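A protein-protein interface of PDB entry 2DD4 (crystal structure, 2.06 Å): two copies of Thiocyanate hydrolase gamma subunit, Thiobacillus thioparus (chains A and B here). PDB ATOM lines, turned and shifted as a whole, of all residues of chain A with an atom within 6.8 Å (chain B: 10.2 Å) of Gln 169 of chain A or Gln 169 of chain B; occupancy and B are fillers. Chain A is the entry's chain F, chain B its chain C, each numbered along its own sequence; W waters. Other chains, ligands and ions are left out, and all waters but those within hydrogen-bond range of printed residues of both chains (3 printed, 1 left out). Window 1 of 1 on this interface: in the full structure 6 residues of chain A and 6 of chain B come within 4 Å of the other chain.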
ATOM      1  N   ARG A 160     -19.685 -23.726  28.149  1.00  0.00           N
ATOM      2  CA  ARG A 160     -18.604 -24.709  28.210  1.00  0.00           C
ATOM      3  C   ARG A 160     -18.073 -24.834  29.637  1.00  0.00           C
ATOM      4  O   ARG A 160     -17.836 -25.939  30.135  1.00  0.00           O
ATOM      5  CB  ARG A 160     -17.457 -24.285  27.294  1.00  0.00           C
ATOM      6  CG  ARG A 160     -17.811 -24.220  25.819  1.00  0.00           C
ATOM      7  CD  ARG A 160     -17.557 -25.541  25.144  1.00  0.00           C
ATOM      8  NE  ARG A 160     -17.919 -25.517  23.730  1.00  0.00           N
ATOM      9  CZ  ARG A 160     -17.675 -26.516  22.892  1.00  0.00           C
ATOM     10  NH1 ARG A 160     -17.069 -27.612  23.331  1.00  0.00           N
ATOM     11  NH2 ARG A 160     -18.041 -26.427  21.619  1.00  0.00           N
ATOM     12  N   LEU A 163     -20.905 -26.290  32.056  1.00  0.00           N
ATOM     13  CA  LEU A 163     -21.059 -27.722  31.805  1.00  0.00           C
ATOM     14  C   LEU A 163     -19.864 -28.495  32.366  1.00  0.00           C
ATOM     15  O   LEU A 163     -20.024 -29.595  32.900  1.00  0.00           O
ATOM     16  CB  LEU A 163     -21.210 -27.989  30.302  1.00  0.00           C
ATOM     17  CG  LEU A 163     -22.527 -27.506  29.681  1.00  0.00           C
ATOM     18  CD1 LEU A 163     -22.516 -27.748  28.179  1.00  0.00           C
ATOM     19  CD2 LEU A 163     -23.698 -28.248  30.331  1.00  0.00           C
ATOM     20  N   ALA A 164     -18.670 -27.918  32.256  1.00  0.00           N
ATOM     21  CA  ALA A 164     -17.473 -28.576  32.779  1.00  0.00           C
ATOM     22  C   ALA A 164     -17.645 -28.765  34.286  1.00  0.00           C
ATOM     23  O   ALA A 164     -17.278 -29.804  34.840  1.00  0.00           O
ATOM     24  CB  ALA A 164     -16.233 -27.739  32.485  1.00  0.00           C
ATOM     25  N   GLY A 167     -19.456 -31.574  35.058  1.00  0.00           N
ATOM     26  CA  GLY A 167     -18.756 -32.789  34.676  1.00  0.00           C
ATOM     27  C   GLY A 167     -18.963 -33.195  33.226  1.00  0.00           C
ATOM     28  O   GLY A 167     -18.672 -34.331  32.845  1.00  0.00           O
ATOM     29  N   LEU A 168     -19.457 -32.270  32.410  1.00  0.00           N
ATOM     30  CA  LEU A 168     -19.695 -32.556  31.001  1.00  0.00           C
ATOM     31  C   LEU A 168     -18.828 -31.697  30.091  1.00  0.00           C
ATOM     32  O   LEU A 168     -18.753 -30.478  30.250  1.00  0.00           O
ATOM     33  CB  LEU A 168     -21.173 -32.334  30.664  1.00  0.00           C
ATOM     34  CG  LEU A 168     -21.592 -32.482  29.198  1.00  0.00           C
ATOM     35  CD1 LEU A 168     -21.309 -33.902  28.708  1.00  0.00           C
ATOM     36  CD2 LEU A 168     -23.074 -32.148  29.063  1.00  0.00           C
ATOM     37  N   GLN A 169     -18.178 -32.341  29.129  1.00  0.00           N
ATOM     38  CA  GLN A 169     -17.324 -31.643  28.179  1.00  0.00           C
ATOM     39  C   GLN A 169     -17.498 -32.247  26.784  1.00  0.00           C
ATOM     40  O   GLN A 169     -17.623 -33.461  26.637  1.00  0.00           O
ATOM     41  CB  GLN A 169     -15.866 -31.739  28.631  1.00  0.00           C
ATOM     42  CG  GLN A 169     -14.861 -31.158  27.658  1.00  0.00           C
ATOM     43  CD  GLN A 169     -13.448 -31.169  28.217  1.00  0.00           C
ATOM     44  OE1 GLN A 169     -13.100 -30.360  29.081  1.00  0.00           O
ATOM     45  NE2 GLN A 169     -12.632 -32.095  27.737  1.00  0.00           N
ATOM     46  N   LEU A 170     -17.523 -31.389  25.768  1.00  0.00           N
ATOM     47  CA  LEU A 170     -17.690 -31.828  24.387  1.00  0.00           C
ATOM     48  C   LEU A 170     -16.574 -31.278  23.509  1.00  0.00           C
ATOM     49  O   LEU A 170     -15.907 -30.308  23.879  1.00  0.00           O
ATOM     50  CB  LEU A 170     -19.047 -31.355  23.856  1.00  0.00           C
ATOM     51  CG  LEU A 170     -20.239 -32.081  24.481  1.00  0.00           C
ATOM     52  CD1 LEU A 170     -21.350 -31.103  24.777  1.00  0.00           C
ATOM     53  CD2 LEU A 170     -20.699 -33.193  23.549  1.00  0.00           C
ATOM     54  N   PRO A 171     -16.343 -31.901  22.339  1.00  0.00           N
ATOM     55  CA  PRO A 171     -15.293 -31.443  21.424  1.00  0.00           C
ATOM     56  C   PRO A 171     -15.500 -29.971  21.103  1.00  0.00           C
ATOM     57  O   PRO A 171     -16.638 -29.506  21.002  1.00  0.00           O
ATOM     58  CB  PRO A 171     -15.489 -32.332  20.199  1.00  0.00           C
ATOM     59  CG  PRO A 171     -16.001 -33.612  20.803  1.00  0.00           C
ATOM     60  CD  PRO A 171     -17.012 -33.104  21.809  1.00  0.00           C
ATOM     61  N   SER A 172     -14.406 -29.240  20.941  1.00  0.00           N
ATOM     62  CA  SER A 172     -14.501 -27.817  20.648  1.00  0.00           C
ATOM     63  C   SER A 172     -15.225 -27.532  19.331  1.00  0.00           C
ATOM     64  O   SER A 172     -15.863 -26.489  19.189  1.00  0.00           O
ATOM     65  CB  SER A 172     -13.105 -27.194  20.630  1.00  0.00           C
ATOM     66  OG  SER A 172     -12.280 -27.834  19.675  1.00  0.00           O
ATOM     67  N   GLU A 173     -15.140 -28.461  18.379  1.00  0.00           N
ATOM     68  CA  GLU A 173     -15.790 -28.283  17.080  1.00  0.00           C
ATOM     69  C   GLU A 173     -17.291 -28.558  17.137  1.00  0.00           C
ATOM     70  O   GLU A 173     -18.035 -28.142  16.249  1.00  0.00           O
ATOM     71  CB  GLU A 173     -15.164 -29.196  16.020  1.00  0.00           C
ATOM     72  CG  GLU A 173     -13.720 -29.569  16.273  1.00  0.00           C
ATOM     73  CD  GLU A 173     -13.582 -30.677  17.304  1.00  0.00           C
ATOM     74  OE1 GLU A 173     -14.200 -31.748  17.111  1.00  0.00           O
ATOM     75  OE2 GLU A 173     -12.855 -30.480  18.301  1.00  0.00           O
ATOM     76  N   ILE A 176     -22.248 -26.306  20.687  1.00  0.00           N
ATOM     77  CA  ILE A 176     -23.004 -26.352  21.927  1.00  0.00           C
ATOM     78  C   ILE A 176     -24.029 -25.246  21.730  1.00  0.00           C
ATOM     79  O   ILE A 176     -23.671 -24.104  21.418  1.00  0.00           O
ATOM     80  CB  ILE A 176     -22.136 -26.043  23.176  1.00  0.00           C
ATOM     81  CG1 ILE A 176     -21.462 -27.318  23.695  1.00  0.00           C
ATOM     82  CG2 ILE A 176     -23.017 -25.489  24.291  1.00  0.00           C
ATOM     83  CD1 ILE A 176     -20.636 -28.046  22.667  1.00  0.00           C
ATOM     84  N   LYS B 123      -0.728 -32.077  31.111  1.00  0.00           N
ATOM     85  CA  LYS B 123      -0.612 -30.724  30.577  1.00  0.00           C
ATOM     86  C   LYS B 123      -0.557 -29.737  31.750  1.00  0.00           C
ATOM     87  O   LYS B 123      -1.430 -29.748  32.621  1.00  0.00           O
ATOM     88  CB  LYS B 123      -1.796 -30.422  29.655  1.00  0.00           C
ATOM     89  CG  LYS B 123      -1.550 -29.262  28.699  1.00  0.00           C
ATOM     90  CD  LYS B 123      -1.883 -27.926  29.337  1.00  0.00           C
ATOM     91  CE  LYS B 123      -1.318 -26.770  28.525  1.00  0.00           C
ATOM     92  NZ  LYS B 123       0.162 -26.703  28.641  1.00  0.00           N
ATOM     93  N   TRP B 158     -10.465 -23.859  39.360  1.00  0.00           N
ATOM     94  CA  TRP B 158     -11.269 -24.117  38.161  1.00  0.00           C
ATOM     95  C   TRP B 158     -10.379 -24.020  36.916  1.00  0.00           C
ATOM     96  O   TRP B 158     -10.687 -23.280  35.979  1.00  0.00           O
ATOM     97  CB  TRP B 158     -12.402 -23.082  38.065  1.00  0.00           C
ATOM     98  CG  TRP B 158     -13.366 -23.117  39.225  1.00  0.00           C
ATOM     99  CD1 TRP B 158     -14.354 -24.036  39.443  1.00  0.00           C
ATOM    100  CD2 TRP B 158     -13.408 -22.210  40.338  1.00  0.00           C
ATOM    101  NE1 TRP B 158     -15.008 -23.759  40.620  1.00  0.00           N
ATOM    102  CE2 TRP B 158     -14.449 -22.646  41.189  1.00  0.00           C
ATOM    103  CE3 TRP B 158     -12.668 -21.075  40.698  1.00  0.00           C
ATOM    104  CZ2 TRP B 158     -14.771 -21.985  42.381  1.00  0.00           C
ATOM    105  CZ3 TRP B 158     -12.988 -20.415  41.886  1.00  0.00           C
ATOM    106  CH2 TRP B 158     -14.032 -20.874  42.711  1.00  0.00           C
ATOM    107  N   PRO B 159      -9.269 -24.778  36.885  1.00  0.00           N
ATOM    108  CA  PRO B 159      -8.353 -24.741  35.737  1.00  0.00           C
ATOM    109  C   PRO B 159      -8.984 -25.063  34.388  1.00  0.00           C
ATOM    110  O   PRO B 159      -8.664 -24.425  33.387  1.00  0.00           O
ATOM    111  CB  PRO B 159      -7.259 -25.737  36.132  1.00  0.00           C
ATOM    112  CG  PRO B 159      -8.005 -26.731  36.987  1.00  0.00           C
ATOM    113  CD  PRO B 159      -8.875 -25.831  37.838  1.00  0.00           C
ATOM    114  N   ARG B 160      -9.877 -26.050  34.362  1.00  0.00           N
ATOM    115  CA  ARG B 160     -10.549 -26.437  33.125  1.00  0.00           C
ATOM    116  C   ARG B 160     -11.363 -25.270  32.575  1.00  0.00           C
ATOM    117  O   ARG B 160     -11.347 -24.994  31.374  1.00  0.00           O
ATOM    118  CB  ARG B 160     -11.488 -27.623  33.377  1.00  0.00           C
ATOM    119  CG  ARG B 160     -10.794 -28.919  33.804  1.00  0.00           C
ATOM    120  CD  ARG B 160     -10.246 -29.676  32.618  1.00  0.00           C
ATOM    121  NE  ARG B 160      -9.578 -30.917  33.008  1.00  0.00           N
ATOM    122  CZ  ARG B 160      -9.209 -31.863  32.149  1.00  0.00           C
ATOM    123  NH1 ARG B 160      -9.450 -31.710  30.855  1.00  0.00           N
ATOM    124  NH2 ARG B 160      -8.593 -32.957  32.576  1.00  0.00           N
ATOM    125  N   GLN B 161     -12.074 -24.589  33.466  1.00  0.00           N
ATOM    126  CA  GLN B 161     -12.907 -23.461  33.082  1.00  0.00           C
ATOM    127  C   GLN B 161     -12.092 -22.247  32.622  1.00  0.00           C
ATOM    128  O   GLN B 161     -12.412 -21.630  31.604  1.00  0.00           O
ATOM    129  CB  GLN B 161     -13.818 -23.069  34.248  1.00  0.00           C
ATOM    130  CG  GLN B 161     -14.862 -24.128  34.635  1.00  0.00           C
ATOM    131  CD  GLN B 161     -14.279 -25.333  35.368  1.00  0.00           C
ATOM    132  OE1 GLN B 161     -13.140 -25.308  35.837  1.00  0.00           O
ATOM    133  NE2 GLN B 161     -15.072 -26.390  35.484  1.00  0.00           N
ATOM    134  N   VAL B 162     -11.045 -21.898  33.367  1.00  0.00           N
ATOM    135  CA  VAL B 162     -10.215 -20.754  32.993  1.00  0.00           C
ATOM    136  C   VAL B 162      -9.495 -21.013  31.666  1.00  0.00           C
ATOM    137  O   VAL B 162      -9.431 -20.129  30.805  1.00  0.00           O
ATOM    138  CB  VAL B 162      -9.173 -20.426  34.093  1.00  0.00           C
ATOM    139  CG1 VAL B 162      -8.253 -19.297  33.627  1.00  0.00           C
ATOM    140  CG2 VAL B 162      -9.893 -20.009  35.375  1.00  0.00           C
ATOM    141  N   LEU B 163      -8.958 -22.220  31.497  1.00  0.00           N
ATOM    142  CA  LEU B 163      -8.261 -22.566  30.256  1.00  0.00           C
ATOM    143  C   LEU B 163      -9.220 -22.521  29.067  1.00  0.00           C
ATOM    144  O   LEU B 163      -8.839 -22.116  27.970  1.00  0.00           O
ATOM    145  CB  LEU B 163      -7.625 -23.957  30.363  1.00  0.00           C
ATOM    146  CG  LEU B 163      -6.399 -24.061  31.274  1.00  0.00           C
ATOM    147  CD1 LEU B 163      -5.902 -25.496  31.308  1.00  0.00           C
ATOM    148  CD2 LEU B 163      -5.303 -23.134  30.763  1.00  0.00           C
ATOM    149  N   ALA B 164     -10.460 -22.946  29.286  1.00  0.00           N
ATOM    150  CA  ALA B 164     -11.469 -22.922  28.231  1.00  0.00           C
ATOM    151  C   ALA B 164     -11.722 -21.467  27.831  1.00  0.00           C
ATOM    152  O   ALA B 164     -11.924 -21.158  26.655  1.00  0.00           O
ATOM    153  CB  ALA B 164     -12.756 -23.569  28.720  1.00  0.00           C
ATOM    154  N   GLU B 165     -11.714 -20.575  28.815  1.00  0.00           N
ATOM    155  CA  GLU B 165     -11.904 -19.154  28.555  1.00  0.00           C
ATOM    156  C   GLU B 165     -10.778 -18.659  27.645  1.00  0.00           C
ATOM    157  O   GLU B 165     -10.984 -17.776  26.810  1.00  0.00           O
ATOM    158  CB  GLU B 165     -11.885 -18.366  29.869  1.00  0.00           C
ATOM    159  CG  GLU B 165     -13.184 -18.398  30.654  1.00  0.00           C
ATOM    160  CD  GLU B 165     -13.022 -17.820  32.051  1.00  0.00           C
ATOM    161  OE1 GLU B 165     -12.215 -16.883  32.219  1.00  0.00           O
ATOM    162  OE2 GLU B 165     -13.706 -18.295  32.980  1.00  0.00           O
ATOM    163  N   PHE B 166      -9.587 -19.231  27.815  1.00  0.00           N
ATOM    164  CA  PHE B 166      -8.429 -18.861  27.003  1.00  0.00           C
ATOM    165  C   PHE B 166      -8.456 -19.573  25.656  1.00  0.00           C
ATOM    166  O   PHE B 166      -7.595 -19.343  24.809  1.00  0.00           O
ATOM    167  CB  PHE B 166      -7.121 -19.219  27.713  1.00  0.00           C
ATOM    168  CG  PHE B 166      -6.642 -18.180  28.688  1.00  0.00           C
ATOM    169  CD1 PHE B 166      -6.995 -18.249  30.030  1.00  0.00           C
ATOM    170  CD2 PHE B 166      -5.809 -17.147  28.265  1.00  0.00           C
ATOM    171  CE1 PHE B 166      -6.524 -17.308  30.939  1.00  0.00           C
ATOM    172  CE2 PHE B 166      -5.331 -16.200  29.164  1.00  0.00           C
ATOM    173  CZ  PHE B 166      -5.687 -16.279  30.504  1.00  0.00           C
ATOM    174  N   GLY B 167      -9.437 -20.453  25.474  1.00  0.00           N
ATOM    175  CA  GLY B 167      -9.560 -21.180  24.224  1.00  0.00           C
ATOM    176  C   GLY B 167      -8.811 -22.500  24.194  1.00  0.00           C
ATOM    177  O   GLY B 167      -8.556 -23.044  23.120  1.00  0.00           O
ATOM    178  N   LEU B 168      -8.457 -23.014  25.368  1.00  0.00           N
ATOM    179  CA  LEU B 168      -7.736 -24.278  25.471  1.00  0.00           C
ATOM    180  C   LEU B 168      -8.550 -25.332  26.213  1.00  0.00           C
ATOM    181  O   LEU B 168      -9.025 -25.099  27.324  1.00  0.00           O
ATOM    182  CB  LEU B 168      -6.401 -24.073  26.194  1.00  0.00           C
ATOM    183  CG  LEU B 168      -5.560 -25.336  26.428  1.00  0.00           C
ATOM    184  CD1 LEU B 168      -5.265 -26.020  25.091  1.00  0.00           C
ATOM    185  CD2 LEU B 168      -4.264 -24.963  27.138  1.00  0.00           C
ATOM    186  N   GLN B 169      -8.702 -26.494  25.592  1.00  0.00           N
ATOM    187  CA  GLN B 169      -9.448 -27.591  26.183  1.00  0.00           C
ATOM    188  C   GLN B 169      -8.669 -28.884  25.961  1.00  0.00           C
ATOM    189  O   GLN B 169      -8.076 -29.081  24.904  1.00  0.00           O
ATOM    190  CB  GLN B 169     -10.830 -27.690  25.528  1.00  0.00           C
ATOM    191  CG  GLN B 169     -11.815 -28.598  26.246  1.00  0.00           C
ATOM    192  CD  GLN B 169     -13.210 -28.540  25.635  1.00  0.00           C
ATOM    193  OE1 GLN B 169     -13.416 -28.952  24.494  1.00  0.00           O
ATOM    194  NE2 GLN B 169     -14.172 -28.021  26.396  1.00  0.00           N
ATOM    195  N   LEU B 170      -8.654 -29.752  26.962  1.00  0.00           N
ATOM    196  CA  LEU B 170      -7.957 -31.025  26.842  1.00  0.00           C
ATOM    197  C   LEU B 170      -8.889 -32.171  27.207  1.00  0.00           C
ATOM    198  O   LEU B 170      -9.914 -31.959  27.858  1.00  0.00           O
ATOM    199  CB  LEU B 170      -6.724 -31.052  27.746  1.00  0.00           C
ATOM    200  CG  LEU B 170      -5.563 -30.199  27.235  1.00  0.00           C
ATOM    201  CD1 LEU B 170      -5.552 -28.857  27.942  1.00  0.00           C
ATOM    202  CD2 LEU B 170      -4.265 -30.937  27.463  1.00  0.00           C
ATOM    203  N   PRO B 171      -8.556 -33.398  26.777  1.00  0.00           N
ATOM    204  CA  PRO B 171      -9.398 -34.558  27.089  1.00  0.00           C
ATOM    205  C   PRO B 171      -9.602 -34.670  28.601  1.00  0.00           C
ATOM    206  O   PRO B 171      -8.704 -34.349  29.383  1.00  0.00           O
ATOM    207  CB  PRO B 171      -8.596 -35.724  26.526  1.00  0.00           C
ATOM    208  CG  PRO B 171      -7.892 -35.101  25.345  1.00  0.00           C
ATOM    209  CD  PRO B 171      -7.418 -33.788  25.923  1.00  0.00           C
ATOM    210  N   SER B 172     -10.781 -35.122  29.008  1.00  0.00           N
ATOM    211  CA  SER B 172     -11.085 -35.251  30.425  1.00  0.00           C
ATOM    212  C   SER B 172     -10.152 -36.218  31.150  1.00  0.00           C
ATOM    213  O   SER B 172      -9.904 -36.060  32.343  1.00  0.00           O
ATOM    214  CB  SER B 172     -12.538 -35.698  30.612  1.00  0.00           C
ATOM    215  OG  SER B 172     -12.751 -36.977  30.045  1.00  0.00           O
ATOM    216  N   GLU B 173      -9.629 -37.213  30.434  1.00  0.00           N
ATOM    217  CA  GLU B 173      -8.736 -38.191  31.053  1.00  0.00           C
ATOM    218  C   GLU B 173      -7.324 -37.640  31.244  1.00  0.00           C
ATOM    219  O   GLU B 173      -6.572 -38.124  32.090  1.00  0.00           O
ATOM    220  CB  GLU B 173      -8.661 -39.465  30.212  1.00  0.00           C
ATOM    221  CG  GLU B 173      -8.067 -39.245  28.832  1.00  0.00           C
ATOM    222  CD  GLU B 173      -9.121 -39.049  27.758  1.00  0.00           C
ATOM    223  OE1 GLU B 173     -10.191 -38.468  28.054  1.00  0.00           O
ATOM    224  OE2 GLU B 173      -8.866 -39.470  26.608  1.00  0.00           O
ATOM    225  N   VAL B 174      -6.964 -36.638  30.450  1.00  0.00           N
ATOM    226  CA  VAL B 174      -5.643 -36.034  30.555  1.00  0.00           C
ATOM    227  C   VAL B 174      -5.487 -35.327  31.898  1.00  0.00           C
ATOM    228  O   VAL B 174      -6.418 -34.690  32.394  1.00  0.00           O
ATOM    229  CB  VAL B 174      -5.403 -35.010  29.424  1.00  0.00           C
ATOM    230  CG1 VAL B 174      -4.118 -34.231  29.684  1.00  0.00           C
ATOM    231  CG2 VAL B 174      -5.309 -35.726  28.091  1.00  0.00           C
ATOM    232  N   GLN B 175      -4.304 -35.449  32.487  1.00  0.00           N
ATOM    233  CA  GLN B 175      -4.032 -34.812  33.763  1.00  0.00           C
ATOM    234  C   GLN B 175      -3.662 -33.341  33.598  1.00  0.00           C
ATOM    235  O   GLN B 175      -2.592 -33.025  33.080  1.00  0.00           O
ATOM    236  CB  GLN B 175      -2.880 -35.523  34.487  1.00  0.00           C
ATOM    237  CG  GLN B 175      -2.494 -34.875  35.821  1.00  0.00           C
ATOM    238  CD  GLN B 175      -1.264 -35.509  36.468  1.00  0.00           C
ATOM    239  OE1 GLN B 175      -0.842 -36.609  36.098  1.00  0.00           O
ATOM    240  NE2 GLN B 175      -0.692 -34.817  37.445  1.00  0.00           N
ATOM    241  N   ILE B 176      -4.548 -32.439  34.004  1.00  0.00           N
ATOM    242  CA  ILE B 176      -4.197 -31.028  33.949  1.00  0.00           C
ATOM    243  C   ILE B 176      -3.566 -30.770  35.309  1.00  0.00           C
ATOM    244  O   ILE B 176      -4.164 -31.066  36.348  1.00  0.00           O
ATOM    245  CB  ILE B 176      -5.421 -30.086  33.773  1.00  0.00           C
ATOM    246  CG1 ILE B 176      -5.853 -30.024  32.304  1.00  0.00           C
ATOM    247  CG2 ILE B 176      -5.039 -28.660  34.182  1.00  0.00           C
ATOM    248  CD1 ILE B 176      -6.202 -31.352  31.712  1.00  0.00           C
ATOM    249  N   GLY B 216       1.277 -21.775  29.832  1.00  0.00           N
ATOM    250  CA  GLY B 216       0.385 -22.921  29.831  1.00  0.00           C
ATOM    251  C   GLY B 216      -1.069 -22.616  29.507  1.00  0.00           C
ATOM    252  O   GLY B 216      -1.910 -23.517  29.543  1.00  0.00           O
ATOM    253  N   VAL B 217      -1.383 -21.361  29.193  1.00  0.00           N
ATOM    254  CA  VAL B 217      -2.762 -21.001  28.868  1.00  0.00           C
ATOM    255  C   VAL B 217      -3.064 -21.204  27.385  1.00  0.00           C
ATOM    256  O   VAL B 217      -4.174 -20.935  26.919  1.00  0.00           O
ATOM    257  CB  VAL B 217      -3.079 -19.538  29.259  1.00  0.00           C
ATOM    258  CG1 VAL B 217      -2.968 -19.374  30.772  1.00  0.00           C
ATOM    259  CG2 VAL B 217      -2.133 -18.584  28.538  1.00  0.00           C
ATOM    260  N   ALA B 218      -2.069 -21.690  26.653  1.00  0.00           N
ATOM    261  CA  ALA B 218      -2.216 -21.963  25.227  1.00  0.00           C
ATOM    262  C   ALA B 218      -1.225 -23.053  24.813  1.00  0.00           C
ATOM    263  O   ALA B 218      -0.273 -23.346  25.541  1.00  0.00           O
ATOM    264  CB  ALA B 218      -1.963 -20.694  24.417  1.00  0.00           C
ATOM    265  N   VAL B 219      -1.464 -23.666  23.657  1.00  0.00           N
ATOM    266  CA  VAL B 219      -0.564 -24.690  23.138  1.00  0.00           C
ATOM    267  C   VAL B 219      -0.048 -24.224  21.782  1.00  0.00           C
ATOM    268  O   VAL B 219      -0.738 -23.501  21.061  1.00  0.00           O
ATOM    269  CB  VAL B 219      -1.261 -26.067  22.971  1.00  0.00           C
ATOM    270  CG1 VAL B 219      -1.531 -26.682  24.337  1.00  0.00           C
ATOM    271  CG2 VAL B 219      -2.551 -25.915  22.180  1.00  0.00           C
ATOM    272  N   LYS B 221       0.846 -23.991  17.908  1.00  0.00           N
ATOM    273  CA  LYS B 221       0.144 -24.412  16.699  1.00  0.00           C
ATOM    274  C   LYS B 221       0.862 -23.869  15.472  1.00  0.00           C
ATOM    275  O   LYS B 221       1.267 -22.706  15.445  1.00  0.00           O
ATOM    276  CB  LYS B 221      -1.286 -23.874  16.695  1.00  0.00           C
ATOM    277  CG  LYS B 221      -2.111 -24.224  17.915  1.00  0.00           C
ATOM    278  CD  LYS B 221      -3.426 -23.456  17.888  1.00  0.00           C
ATOM    279  CE  LYS B 221      -4.259 -23.715  19.134  1.00  0.00           C
ATOM    280  NZ  LYS B 221      -5.500 -22.884  19.142  1.00  0.00           N
HETATM  281  O   HOH W   1     -10.329 -29.170  29.305  1.00  0.00           O
HETATM  282  O   HOH W   2     -14.663 -25.346  30.818  1.00  0.00           O
HETATM  283  O   HOH W   3     -14.061 -27.434  29.035  1.00  0.00           O
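Water W3 bridges NE2 of Gln 169 of chain B (2.7 Å) and OE1 of Gln 169 of chain A (3.1 Å).
Water W1 lies within hydrogen-bond range of N of Leu 170 of chain B (2.9 Å), OE1 of Gln 169 of chain A (3.0 Å) and NH1 of Arg 160 of chain B (3.1 Å).
Water W2 bridges the backbone carbonyl oxygen of Arg 160 of chain A (3.3 Å) and the backbone carbonyl oxygen of Arg 160 of chain B (3.4 Å).
The backbone carbonyl oxygen (O) of Trp 158 of chain B sits close to the side-chain amide oxygen (OE1) of Gln 161 of chain B (3.2 Å).
The backbone carbonyl oxygen (O) of Leu 170 of chain B is in hydrogen-bond range of the guanidinium group (NH1) of Arg 160 of chain B (3.0 Å).
NH2 of Arg 160 of chain B lies within hydrogen-bond range of O of Ser 172 of chain B.
NH1 of Arg 160 of chain A lies within hydrogen-bond range of O of Leu 170 of chain A (3.0 Å).
NH2 of Arg 160 of chain A sits at hydrogen-bond distance from O of Ser 172 of chain A (3.3 Å).
The side-chain hydroxyl (OG) of Ser 172 of chain A is in hydrogen-bond range of the side-chain carboxylate (OE2) of Glu 173 of chain A (3.0 Å).
Of the printed residues of chain B, Ala 164 of chain A touches Gln 161 (3.5 Å).
Printed residues of chain B within 4 Å of Gln 169 of chain A: Gln 169, Leu 170 and Ser 172.
No residue of chain B comes within 4 Å of Pro 171 of chain A.
Printed residues of chain B within 4 Å of Ser 172 of chain A: Gln 169.
Of the printed residues of chain A, Gln 161 of chain B touches Ala 164 (3.5 Å).
Printed residues of chain A within 4 Å of Gln 169 of chain B: Gln 169 (3.5 Å), Leu 170 (2.9 Å) and Ser 172 (3.7 Å).
Of the printed residues of chain A, Leu 170 of chain B touches Gln 169.
Of the printed residues of chain A, Ser 172 of chain B touches Gln 169 (3.8 Å).
Gln 161 of chain B touches Ala 164 of chain A (NE2 to CB, 3.5 Å).
CG of Gln 169 of chain A touches NE2 of Gln 169 of chain B, at 3.5 Å.
Gln 169 of chain A touches Ser 172 of chain B (NE2 to N, 3.8 Å).
Gln 169 of chain B touches Ser 172 of chain A.
Printed residues of chain B that touch a printed residue of chain A: Gln 161, Gln 169, Leu 170 and Ser 172.
Of the 11 printed residues of chain A, 4 touch a printed residue of chain B.
Hydrophobic or aromatic side chains of chain A that line the printed part of chain B: Ala 164.
Among the printed residues, no Asp or Glu carboxylate lies within 4 Å of a Lys or Arg side-chain nitrogen of the other chain.
Gln 169 of chain A touches its own counterpart, Gln 169 of chain B.
Gln 169 of chain A touches Leu 170 of chain B, and with the chains exchanged Leu 170 of chain A touches Gln 169 of chain B.
Gln 169 of chain A touches Ser 172 of chain B, and with the chains exchanged Ser 172 of chain A touches Gln 169 of chain B.
OE1 of Gln 169 of chain B sits close to O of Leu 170 of chain A.
O of Leu 170 of chain B sits at hydrogen-bond distance from NE2 of Gln 169 of chain A (2.7 Å).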
